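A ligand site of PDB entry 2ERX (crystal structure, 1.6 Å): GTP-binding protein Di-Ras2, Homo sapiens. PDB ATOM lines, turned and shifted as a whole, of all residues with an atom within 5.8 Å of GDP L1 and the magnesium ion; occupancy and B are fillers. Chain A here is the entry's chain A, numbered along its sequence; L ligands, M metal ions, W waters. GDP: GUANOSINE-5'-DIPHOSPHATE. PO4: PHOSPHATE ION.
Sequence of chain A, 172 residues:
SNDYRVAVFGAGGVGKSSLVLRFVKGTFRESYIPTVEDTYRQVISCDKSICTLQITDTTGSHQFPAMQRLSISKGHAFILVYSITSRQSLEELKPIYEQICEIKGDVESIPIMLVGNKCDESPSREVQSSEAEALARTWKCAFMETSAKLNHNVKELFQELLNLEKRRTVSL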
ATOM      1  N   GLY A  10     -10.523 -17.805  14.008  1.00  0.00           N
ATOM      2  CA  GLY A  10     -11.302 -16.991  13.095  1.00  0.00           C
ATOM      3  C   GLY A  10     -11.068 -15.509  13.310  1.00  0.00           C
ATOM      4  O   GLY A  10     -10.416 -15.107  14.277  1.00  0.00           O
ATOM      5  N   ALA A  11     -11.560 -14.713  12.371  1.00  0.00           N
ATOM      6  CA  ALA A  11     -11.384 -13.245  12.419  1.00  0.00           C
ATOM      7  C   ALA A  11     -12.014 -12.593  13.645  1.00  0.00           C
ATOM      8  O   ALA A  11     -12.896 -13.128  14.243  1.00  0.00           O
ATOM      9  CB  ALA A  11     -11.986 -12.649  11.187  1.00  0.00           C
ATOM     10  N   GLY A  12     -11.591 -11.373  13.969  1.00  0.00           N
ATOM     11  CA  GLY A  12     -12.225 -10.702  15.095  1.00  0.00           C
ATOM     12  C   GLY A  12     -13.690 -10.460  14.734  1.00  0.00           C
ATOM     13  O   GLY A  12     -14.045 -10.093  13.575  1.00  0.00           O
ATOM     14  N   GLY A  13     -14.536 -10.668  15.737  1.00  0.00           N
ATOM     15  CA  GLY A  13     -15.913 -10.275  15.717  1.00  0.00           C
ATOM     16  C   GLY A  13     -16.878 -11.302  15.151  1.00  0.00           C
ATOM     17  O   GLY A  13     -18.073 -11.020  15.050  1.00  0.00           O
ATOM     18  N   VAL A  14     -16.386 -12.479  14.795  1.00  0.00           N
ATOM     19  CA  VAL A  14     -17.261 -13.522  14.221  1.00  0.00           C
ATOM     20  C   VAL A  14     -18.114 -14.305  15.191  1.00  0.00           C
ATOM     21  O   VAL A  14     -19.066 -14.922  14.773  1.00  0.00           O
ATOM     22  CB  VAL A  14     -16.451 -14.488  13.329  1.00  0.00           C
ATOM     23  CG1 VAL A  14     -15.767 -13.702  12.207  1.00  0.00           C
ATOM     24  CG2 VAL A  14     -15.493 -15.314  14.126  1.00  0.00           C
ATOM     25  N   GLY A  15     -17.736 -14.307  16.461  1.00  0.00           N
ATOM     26  CA  GLY A  15     -18.403 -15.058  17.499  1.00  0.00           C
ATOM     27  C   GLY A  15     -17.681 -16.229  18.122  1.00  0.00           C
ATOM     28  O   GLY A  15     -18.319 -17.087  18.754  1.00  0.00           O
ATOM     29  N   LYS A  16     -16.356 -16.266  18.011  1.00  0.00           N
ATOM     30  CA  LYS A  16     -15.542 -17.325  18.649  1.00  0.00           C
ATOM     31  C   LYS A  16     -15.846 -17.389  20.152  1.00  0.00           C
ATOM     32  O   LYS A  16     -16.199 -18.411  20.721  1.00  0.00           O
ATOM     33  CB  LYS A  16     -14.030 -17.101  18.432  1.00  0.00           C
ATOM     34  CG  LYS A  16     -13.560 -17.123  16.983  1.00  0.00           C
ATOM     35  CD  LYS A  16     -12.116 -16.857  16.845  1.00  0.00           C
ATOM     36  CE  LYS A  16     -11.566 -15.594  17.373  1.00  0.00           C
ATOM     37  NZ  LYS A  16     -12.141 -14.392  16.740  1.00  0.00           N
ATOM     38  N   SER A  17     -15.610 -16.254  20.840  1.00  0.00           N
ATOM     39  CA  SER A  17     -15.802 -16.240  22.263  1.00  0.00           C
ATOM     40  C   SER A  17     -17.240 -16.575  22.648  1.00  0.00           C
ATOM     41  O   SER A  17     -17.506 -17.283  23.618  1.00  0.00           O
ATOM     42  CB  SER A  17     -15.389 -14.881  22.826  1.00  0.00           C
ATOM     43  OG  SER A  17     -14.011 -14.649  22.629  1.00  0.00           O
ATOM     44  N   SER A  18     -18.194 -16.013  21.896  1.00  0.00           N
ATOM     45  CA  SER A  18     -19.594 -16.265  22.158  1.00  0.00           C
ATOM     46  C   SER A  18     -20.019 -17.724  22.007  1.00  0.00           C
ATOM     47  O   SER A  18     -20.815 -18.214  22.813  1.00  0.00           O
ATOM     48  CB  SER A  18     -20.491 -15.402  21.254  1.00  0.00           C
ATOM     49  OG  SER A  18     -20.318 -14.002  21.547  1.00  0.00           O
ATOM     50  N   LEU A  19     -19.450 -18.409  21.033  1.00  0.00           N
ATOM     51  CA  LEU A  19     -19.777 -19.841  20.862  1.00  0.00           C
ATOM     52  C   LEU A  19     -19.230 -20.628  22.050  1.00  0.00           C
ATOM     53  O   LEU A  19     -19.913 -21.467  22.658  1.00  0.00           O
ATOM     54  CB  LEU A  19     -19.261 -20.428  19.566  1.00  0.00           C
ATOM     55  CG  LEU A  19     -20.064 -20.025  18.307  1.00  0.00           C
ATOM     56  CD1 LEU A  19     -19.296 -20.339  17.021  1.00  0.00           C
ATOM     57  CD2 LEU A  19     -21.414 -20.731  18.300  1.00  0.00           C
ATOM     58  N   PHE A  28     -24.715 -15.495  27.081  1.00  0.00           N
ATOM     59  CA  PHE A  28     -24.506 -14.678  25.894  1.00  0.00           C
ATOM     60  C   PHE A  28     -24.473 -13.193  26.230  1.00  0.00           C
ATOM     61  O   PHE A  28     -25.319 -12.730  26.993  1.00  0.00           O
ATOM     62  CB  PHE A  28     -25.581 -14.921  24.811  1.00  0.00           C
ATOM     63  CG  PHE A  28     -25.390 -14.096  23.540  1.00  0.00           C
ATOM     64  CD1 PHE A  28     -24.412 -14.434  22.605  1.00  0.00           C
ATOM     65  CD2 PHE A  28     -26.107 -12.990  23.308  1.00  0.00           C
ATOM     66  CE1 PHE A  28     -24.241 -13.658  21.435  1.00  0.00           C
ATOM     67  CE2 PHE A  28     -25.911 -12.241  22.158  1.00  0.00           C
ATOM     68  CZ  PHE A  28     -24.987 -12.561  21.259  1.00  0.00           C
ATOM     69  N   ARG A  29     -23.544 -12.474  25.663  1.00  0.00           N
ATOM     70  CA  ARG A  29     -23.493 -10.985  25.817  1.00  0.00           C
ATOM     71  C   ARG A  29     -23.438 -10.307  24.465  1.00  0.00           C
ATOM     72  O   ARG A  29     -22.734 -10.772  23.563  1.00  0.00           O
ATOM     73  CB  ARG A  29     -22.327 -10.558  26.701  1.00  0.00           C
ATOM     74  CG  ARG A  29     -20.998 -10.989  26.200  1.00  0.00           C
ATOM     75  CD  ARG A  29     -19.790 -10.204  26.805  1.00  0.00           C
ATOM     76  NE  ARG A  29     -18.665 -10.729  26.037  1.00  0.00           N
ATOM     77  CZ  ARG A  29     -17.823 -11.683  26.431  1.00  0.00           C
ATOM     78  NH1 ARG A  29     -17.842 -12.161  27.691  1.00  0.00           N
ATOM     79  NH2 ARG A  29     -16.917 -12.136  25.545  1.00  0.00           N
ATOM     80  N   GLU A  30     -24.179  -9.206  24.321  1.00  0.00           N
ATOM     81  CA  GLU A  30     -24.121  -8.412  23.104  1.00  0.00           C
ATOM     82  C   GLU A  30     -22.848  -7.592  23.026  1.00  0.00           C
ATOM     83  O   GLU A  30     -22.473  -7.164  21.931  1.00  0.00           O
ATOM     84  CB  GLU A  30     -25.325  -7.469  23.017  1.00  0.00           C
ATOM     85  CG  GLU A  30     -26.701  -8.173  23.119  1.00  0.00           C
ATOM     86  CD  GLU A  30     -27.333  -8.525  21.784  1.00  0.00           C
ATOM     87  OE1 GLU A  30     -26.710  -8.306  20.713  1.00  0.00           O
ATOM     88  OE2 GLU A  30     -28.481  -9.046  21.793  1.00  0.00           O
ATOM     89  N   SER A  31     -22.249  -7.250  24.169  1.00  0.00           N
ATOM     90  CA  SER A  31     -21.001  -6.480  24.150  1.00  0.00           C
ATOM     91  C   SER A  31     -19.841  -7.281  23.626  1.00  0.00           C
ATOM     92  O   SER A  31     -19.708  -8.449  23.901  1.00  0.00           O
ATOM     93  CB  SER A  31     -20.618  -5.914  25.543  1.00  0.00           C
ATOM     94  OG  SER A  31     -21.631  -5.063  26.009  1.00  0.00           O
ATOM     95  N   TYR A  32     -19.024  -6.626  22.802  1.00  0.00           N
ATOM     96  CA  TYR A  32     -17.798  -7.215  22.265  1.00  0.00           C
ATOM     97  C   TYR A  32     -16.624  -6.920  23.199  1.00  0.00           C
ATOM     98  O   TYR A  32     -16.293  -5.774  23.473  1.00  0.00           O
ATOM     99  CB  TYR A  32     -17.483  -6.560  20.923  1.00  0.00           C
ATOM    100  CG  TYR A  32     -16.167  -6.915  20.300  1.00  0.00           C
ATOM    101  CD1 TYR A  32     -15.734  -8.244  20.226  1.00  0.00           C
ATOM    102  CD2 TYR A  32     -15.333  -5.946  19.803  1.00  0.00           C
ATOM    103  CE1 TYR A  32     -14.513  -8.569  19.644  1.00  0.00           C
ATOM    104  CE2 TYR A  32     -14.115  -6.262  19.181  1.00  0.00           C
ATOM    105  CZ  TYR A  32     -13.702  -7.572  19.118  1.00  0.00           C
ATOM    106  OH  TYR A  32     -12.489  -7.893  18.525  1.00  0.00           O
ATOM    107  N   ILE A  33     -15.988  -7.992  23.660  1.00  0.00           N
ATOM    108  CA  ILE A  33     -14.833  -7.904  24.501  1.00  0.00           C
ATOM    109  C   ILE A  33     -13.705  -8.650  23.817  1.00  0.00           C
ATOM    110  O   ILE A  33     -13.692  -9.881  23.834  1.00  0.00           O
ATOM    111  CB  ILE A  33     -15.135  -8.540  25.901  1.00  0.00           C
ATOM    112  CG1 ILE A  33     -16.404  -7.953  26.522  1.00  0.00           C
ATOM    113  CG2 ILE A  33     -13.876  -8.376  26.784  1.00  0.00           C
ATOM    114  CD1 ILE A  33     -16.773  -8.470  27.912  1.00  0.00           C
ATOM    115  N   PRO A  34     -12.752  -7.964  23.197  1.00  0.00           N
ATOM    116  CA  PRO A  34     -11.631  -8.589  22.522  1.00  0.00           C
ATOM    117  C   PRO A  34     -10.862  -9.584  23.370  1.00  0.00           C
ATOM    118  O   PRO A  34     -10.669  -9.350  24.558  1.00  0.00           O
ATOM    119  CB  PRO A  34     -10.735  -7.442  22.079  1.00  0.00           C
ATOM    120  CG  PRO A  34     -11.668  -6.264  21.988  1.00  0.00           C
ATOM    121  CD  PRO A  34     -12.711  -6.491  23.068  1.00  0.00           C
ATOM    122  N   THR A  35     -10.430 -10.670  22.732  1.00  0.00           N
ATOM    123  CA  THR A  35      -9.733 -11.719  23.414  1.00  0.00           C
ATOM    124  C   THR A  35      -8.237 -11.702  23.013  1.00  0.00           C
ATOM    125  O   THR A  35      -7.902 -11.325  21.881  1.00  0.00           O
ATOM    126  CB  THR A  35     -10.290 -13.093  22.988  1.00  0.00           C
ATOM    127  OG1 THR A  35     -11.747 -13.068  22.951  1.00  0.00           O
ATOM    128  CG2 THR A  35      -9.789 -14.217  23.829  1.00  0.00           C
ATOM    129  N   ASP A  57      -9.855 -20.421  23.119  1.00  0.00           N
ATOM    130  CA  ASP A  57     -10.533 -19.365  22.391  1.00  0.00           C
ATOM    131  C   ASP A  57      -9.427 -18.349  22.011  1.00  0.00           C
ATOM    132  O   ASP A  57      -8.869 -17.728  22.888  1.00  0.00           O
ATOM    133  CB  ASP A  57     -11.512 -18.663  23.401  1.00  0.00           C
ATOM    134  CG  ASP A  57     -12.252 -17.525  22.801  1.00  0.00           C
ATOM    135  OD1 ASP A  57     -12.364 -17.477  21.554  1.00  0.00           O
ATOM    136  OD2 ASP A  57     -12.784 -16.695  23.643  1.00  0.00           O
ATOM    137  N   THR A  58      -9.048 -18.325  20.730  1.00  0.00           N
ATOM    138  CA  THR A  58      -7.906 -17.543  20.272  1.00  0.00           C
ATOM    139  C   THR A  58      -8.307 -16.132  19.861  1.00  0.00           C
ATOM    140  O   THR A  58      -9.469 -15.745  19.888  1.00  0.00           O
ATOM    141  CB  THR A  58      -7.207 -18.259  19.087  1.00  0.00           C
ATOM    142  OG1 THR A  58      -8.070 -18.196  17.973  1.00  0.00           O
ATOM    143  CG2 THR A  58      -6.856 -19.720  19.460  1.00  0.00           C
ATOM    144  N   ASN A 117     -21.202 -18.735  11.741  1.00  0.00           N
ATOM    145  CA  ASN A 117     -21.943 -18.208  12.864  1.00  0.00           C
ATOM    146  C   ASN A 117     -22.834 -17.013  12.506  1.00  0.00           C
ATOM    147  O   ASN A 117     -22.741 -16.460  11.416  1.00  0.00           O
ATOM    148  CB  ASN A 117     -21.002 -17.877  14.022  1.00  0.00           C
ATOM    149  CG  ASN A 117     -21.705 -17.575  15.338  1.00  0.00           C
ATOM    150  OD1 ASN A 117     -22.635 -18.272  15.795  1.00  0.00           O
ATOM    151  ND2 ASN A 117     -21.305 -16.439  15.951  1.00  0.00           N
ATOM    152  N   LYS A 118     -23.725 -16.647  13.420  1.00  0.00           N
ATOM    153  CA  LYS A 118     -24.669 -15.520  13.225  1.00  0.00           C
ATOM    154  C   LYS A 118     -25.785 -15.837  12.226  1.00  0.00           C
ATOM    155  O   LYS A 118     -26.307 -14.966  11.542  1.00  0.00           O
ATOM    156  CB  LYS A 118     -23.957 -14.198  12.854  1.00  0.00           C
ATOM    157  CG  LYS A 118     -22.838 -13.775  13.781  1.00  0.00           C
ATOM    158  CD  LYS A 118     -22.466 -12.313  13.675  1.00  0.00           C
ATOM    159  CE  LYS A 118     -21.261 -11.973  14.571  1.00  0.00           C
ATOM    160  NZ  LYS A 118     -20.889 -10.523  14.525  1.00  0.00           N
ATOM    161  N   CYS A 119     -26.162 -17.113  12.168  1.00  0.00           N
ATOM    162  CA  CYS A 119     -27.186 -17.530  11.227  1.00  0.00           C
ATOM    163  C   CYS A 119     -28.580 -16.916  11.544  1.00  0.00           C
ATOM    164  O   CYS A 119     -29.470 -16.866  10.669  1.00  0.00           O
ATOM    165  CB  CYS A 119     -27.119 -19.050  11.077  1.00  0.00           C
ATOM    166  SG  CYS A 119     -27.849 -19.974  12.404  1.00  0.00           S
ATOM    167  N   ASP A 120     -28.741 -16.380  12.746  1.00  0.00           N
ATOM    168  CA  ASP A 120     -29.885 -15.483  13.033  1.00  0.00           C
ATOM    169  C   ASP A 120     -29.957 -14.204  12.160  1.00  0.00           C
ATOM    170  O   ASP A 120     -31.037 -13.578  12.027  1.00  0.00           O
ATOM    171  CB  ASP A 120     -29.916 -15.117  14.526  1.00  0.00           C
ATOM    172  CG  ASP A 120     -28.683 -14.340  14.949  1.00  0.00           C
ATOM    173  OD1 ASP A 120     -27.633 -15.008  15.048  1.00  0.00           O
ATOM    174  OD2 ASP A 120     -28.780 -13.117  15.215  1.00  0.00           O
ATOM    175  N   GLU A 121     -28.829 -13.779  11.604  1.00  0.00           N
ATOM    176  CA  GLU A 121     -28.721 -12.599  10.744  1.00  0.00           C
ATOM    177  C   GLU A 121     -28.782 -12.968   9.255  1.00  0.00           C
ATOM    178  O   GLU A 121     -28.225 -12.260   8.375  1.00  0.00           O
ATOM    179  CB  GLU A 121     -27.426 -11.847  11.008  1.00  0.00           C
ATOM    180  CG  GLU A 121     -27.225 -11.361  12.469  1.00  0.00           C
ATOM    181  CD  GLU A 121     -27.972 -10.127  12.802  1.00  0.00           C
ATOM    182  OE1 GLU A 121     -27.451  -9.371  13.687  1.00  0.00           O
ATOM    183  OE2 GLU A 121     -29.075  -9.862  12.219  1.00  0.00           O
ATOM    184  N   THR A 146     -24.284 -21.887  12.851  1.00  0.00           N
ATOM    185  CA  THR A 146     -24.662 -21.741  14.256  1.00  0.00           C
ATOM    186  C   THR A 146     -25.209 -20.349  14.528  1.00  0.00           C
ATOM    187  O   THR A 146     -24.971 -19.423  13.767  1.00  0.00           O
ATOM    188  CB  THR A 146     -23.446 -21.917  15.173  1.00  0.00           C
ATOM    189  OG1 THR A 146     -22.421 -20.970  14.808  1.00  0.00           O
ATOM    190  CG2 THR A 146     -22.876 -23.322  15.006  1.00  0.00           C
ATOM    191  N   SER A 147     -25.826 -20.199  15.696  1.00  0.00           N
ATOM    192  CA  SER A 147     -26.052 -18.910  16.261  1.00  0.00           C
ATOM    193  C   SER A 147     -25.808 -18.978  17.764  1.00  0.00           C
ATOM    194  O   SER A 147     -26.577 -19.572  18.515  1.00  0.00           O
ATOM    195  CB  SER A 147     -27.450 -18.360  16.019  1.00  0.00           C
ATOM    196  OG  SER A 147     -27.672 -17.165  16.692  1.00  0.00           O
ATOM    197  N   ALA A 148     -24.753 -18.323  18.207  1.00  0.00           N
ATOM    198  CA  ALA A 148     -24.528 -18.201  19.638  1.00  0.00           C
ATOM    199  C   ALA A 148     -25.684 -17.449  20.308  1.00  0.00           C
ATOM    200  O   ALA A 148     -26.049 -17.750  21.428  1.00  0.00           O
ATOM    201  CB  ALA A 148     -23.205 -17.564  19.906  1.00  0.00           C
ATOM    202  N   LYS A 149     -26.190 -16.418  19.635  1.00  0.00           N
ATOM    203  CA  LYS A 149     -27.248 -15.589  20.182  1.00  0.00           C
ATOM    204  C   LYS A 149     -28.496 -16.386  20.443  1.00  0.00           C
ATOM    205  O   LYS A 149     -29.125 -16.233  21.497  1.00  0.00           O
ATOM    206  CB  LYS A 149     -27.546 -14.421  19.239  1.00  0.00           C
ATOM    207  CG  LYS A 149     -28.565 -13.448  19.767  1.00  0.00           C
ATOM    208  CD  LYS A 149     -28.530 -12.155  18.935  1.00  0.00           C
ATOM    209  CE  LYS A 149     -29.591 -11.205  19.389  1.00  0.00           C
ATOM    210  NZ  LYS A 149     -29.808 -10.168  18.355  1.00  0.00           N
ATOM    211  N   LEU A 150     -28.884 -17.175  19.462  1.00  0.00           N
ATOM    212  CA  LEU A 150     -30.085 -18.011  19.590  1.00  0.00           C
ATOM    213  C   LEU A 150     -29.893 -19.350  20.298  1.00  0.00           C
ATOM    214  O   LEU A 150     -30.856 -20.050  20.574  1.00  0.00           O
ATOM    215  CB  LEU A 150     -30.616 -18.286  18.182  1.00  0.00           C
ATOM    216  CG  LEU A 150     -31.529 -17.360  17.432  1.00  0.00           C
ATOM    217  CD1 LEU A 150     -32.065 -18.143  16.220  1.00  0.00           C
ATOM    218  CD2 LEU A 150     -32.692 -16.970  18.283  1.00  0.00           C
HETATM  219  PB  GDP L   1     -14.888 -13.002  18.583  1.00  0.00           P
HETATM  220  O1B GDP L   1     -14.857 -13.939  17.348  1.00  0.00           O
HETATM  221  O2B GDP L   1     -14.241 -11.682  18.304  1.00  0.00           O
HETATM  222  O3B GDP L   1     -14.459 -13.643  19.860  1.00  0.00           O
HETATM  223  O3A GDP L   1     -16.489 -12.680  18.709  1.00  0.00           O
HETATM  224  PA  GDP L   1     -17.365 -12.345  19.980  1.00  0.00           P
HETATM  225  O1A GDP L   1     -16.617 -11.439  20.890  1.00  0.00           O
HETATM  226  O2A GDP L   1     -17.823 -13.578  20.627  1.00  0.00           O
HETATM  227  O5' GDP L   1     -18.651 -11.631  19.323  1.00  0.00           O
HETATM  228  C5' GDP L   1     -18.378 -10.464  18.571  1.00  0.00           C
HETATM  229  C4' GDP L   1     -19.708  -9.682  18.526  1.00  0.00           C
HETATM  230  O4' GDP L   1     -20.703 -10.469  17.792  1.00  0.00           O
HETATM  231  C3' GDP L   1     -20.375  -9.479  19.861  1.00  0.00           C
HETATM  232  O3' GDP L   1     -21.096  -8.208  19.782  1.00  0.00           O
HETATM  233  C2' GDP L   1     -21.409 -10.592  20.030  1.00  0.00           C
HETATM  234  O2' GDP L   1     -22.614 -10.261  20.780  1.00  0.00           O
HETATM  235  C1' GDP L   1     -21.813 -10.814  18.561  1.00  0.00           C
HETATM  236  N9  GDP L   1     -22.298 -12.162  18.286  1.00  0.00           N
HETATM  237  C8  GDP L   1     -21.647 -13.351  18.553  1.00  0.00           C
HETATM  238  N7  GDP L   1     -22.333 -14.436  18.116  1.00  0.00           N
HETATM  239  C5  GDP L   1     -23.471 -13.924  17.541  1.00  0.00           C
HETATM  240  C6  GDP L   1     -24.617 -14.538  16.925  1.00  0.00           C
HETATM  241  O6  GDP L   1     -24.683 -15.811  16.828  1.00  0.00           O
HETATM  242  N1  GDP L   1     -25.541 -13.666  16.410  1.00  0.00           N
HETATM  243  C2  GDP L   1     -25.449 -12.334  16.512  1.00  0.00           C
HETATM  244  N2  GDP L   1     -26.445 -11.613  15.957  1.00  0.00           N
HETATM  245  N3  GDP L   1     -24.446 -11.673  17.101  1.00  0.00           N
HETATM  246  C4  GDP L   1     -23.437 -12.475  17.644  1.00  0.00           C
HETATM  247  P   PO4 L   2     -11.045 -11.518  19.157  1.00  0.00           P
HETATM  248  O1  PO4 L   2     -10.696 -12.386  17.957  1.00  0.00           O
HETATM  249  O2  PO4 L   2     -11.632 -12.234  20.298  1.00  0.00           O
HETATM  250  O3  PO4 L   2      -9.885 -10.644  19.533  1.00  0.00           O
HETATM  251  O4  PO4 L   2     -12.045 -10.439  18.759  1.00  0.00           O
HETATM  252 MG    MG M   1     -13.003 -13.346  21.285  1.00  0.00          MG
HETATM  253  O   HOH W   1     -17.351 -10.553  23.315  1.00  0.00           O
HETATM  254  O   HOH W   2     -14.118 -11.748  21.899  1.00  0.00           O
HETATM  255  O   HOH W   3     -23.417  -9.313  15.725  1.00  0.00           O
HETATM  256  O   HOH W   4     -11.953 -15.064  20.741  1.00  0.00           O
HETATM  257  O   HOH W   5     -27.014  -8.927  16.995  1.00  0.00           O
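O2A of GDP L1 sits at hydrogen-bond distance from N of Ser 17 (3.5 Å). N of Ser 18 sits at hydrogen-bond distance from O2A of GDP L1, at 2.8 Å. O2A of GDP L1 sits at hydrogen-bond distance from OG of Ser 18. The backbone carbonyl oxygen (O) of Glu 30 is in hydrogen-bond range of an oxygen (O3') of GDP L1, at 2.8 Å. The backbone NH (N) of Gly 13 lies within hydrogen-bond range of an oxygen (O2B) of GDP L1, at 2.8 Å. The backbone NH (N) of Lys 16 is in hydrogen-bond range of an oxygen (O1B) of GDP L1 (2.8 Å). The side-chain amino group (NZ) of Lys 16 lies within salt-bridge range of an oxygen (O1B) of GDP L1 (2.8 Å). O of Arg 29 lies within hydrogen-bond range of O2' of GDP L1 (2.8 Å). N1 of GDP L1 lies within hydrogen-bond range of OD1 of Asp 120 (2.8 Å). N of Ala 148 lies within hydrogen-bond range of O6 of GDP L1 (2.9 Å). An oxygen (O1B) of GDP L1 sits at hydrogen-bond distance from the backbone NH (N) of Gly 15 (3.0 Å). The side-chain amide nitrogen (ND2) of Asn 117 is in hydrogen-bond range of a nitrogen (N7) of GDP L1 (3.1 Å). The backbone NH (N) of Lys 149 sits at hydrogen-bond distance from an oxygen (O6) of GDP L1 (3.2 Å). The side-chain amino group of Lys 118 is in hydrogen-bond range of an oxygen (O4') of GDP L1 (3.3 Å). The side-chain hydroxyl (OG) of Ser 147 is in hydrogen-bond range of an oxygen (O6) of GDP L1, at 3.3 Å. An oxygen (O1B) of GDP L1 lies within hydrogen-bond range of the backbone NH of Val 14, at 3.3 Å. OE1 of Glu 121 lies within hydrogen-bond range of N2 of GDP L1 (3.3 Å).
Ala 11 touches GDP L1. C of Gly 12 touches O2B of GDP L1, 3.8 Å away. Phe 28 touches GDP L1 (CZ to O2', 3.3 Å). CD1 of Tyr 32 touches O1A of GDP L1, at 3.4 Å. The nearest printed residue that does not touch GDP L1 is Ser 31 (4.1 Å).
Water W4 bridges OD1 of Asp 57 (2.6 Å) and O of Thr 58 (2.7 Å). Water W2 lies within hydrogen-bond range of an oxygen (O1A) of GDP L1 (2.7 Å) and the backbone carbonyl oxygen of Ile 33 (2.7 Å). Water W1 lies within hydrogen-bond range of an oxygen (O1A) of GDP L1 (2.7 Å), the guanidinium group of Arg 29 (2.8 Å), the backbone NH of Ile 33 (2.9 Å) and the backbone carbonyl oxygen of Ser 31 (3.2 Å). Water W3 lies within hydrogen-bond range of N3 of GDP L1 (2.9 Å) and NZ of Lys 118 (3.0 Å). Water W5 lies within hydrogen-bond range of a nitrogen (N2) of GDP L1, the side-chain amino group (NZ) of Lys 149 and the side-chain carboxylate (OE1) of Glu 121.
The magnesium ion is bound by O2 of PO4 L2 (2.0 Å), water W2 (2.0 Å), O3B of GDP L1 (2.1 Å), water W4 (2.1 Å), OG1 of Thr 35 (2.1 Å) and OG of Ser 17 (2.1 Å). The magnesium ion has six donor atoms within binding distance.
The side-chain hydroxyl (OG) of Ser 17 lies close to the side-chain carboxylate (OD2) of Asp 57 (2.6 Å). OE2 of Glu 30 is in salt-bridge range of NZ of Lys 149, at 3.9 Å. The side-chain amino group (NZ) of Lys 16 sits at hydrogen-bond distance from the backbone carbonyl oxygen (O) of Ala 11 (2.9 Å). NE of Arg 29 lies within hydrogen-bond range of O of Ser 31 (3.3 Å). The side-chain carboxylate of Asp 120 sits at hydrogen-bond distance from the side-chain hydroxyl of Ser 147 (2.7 Å). The backbone NH of Ala 148 sits at hydrogen-bond distance from the side-chain amide oxygen of Asn 117. The side-chain amide nitrogen (ND2) of Asn 117 lies within hydrogen-bond range of the backbone carbonyl oxygen (O) of Val 14 (2.9 Å). OG of Ser 147 lies within hydrogen-bond range of N of Leu 150.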
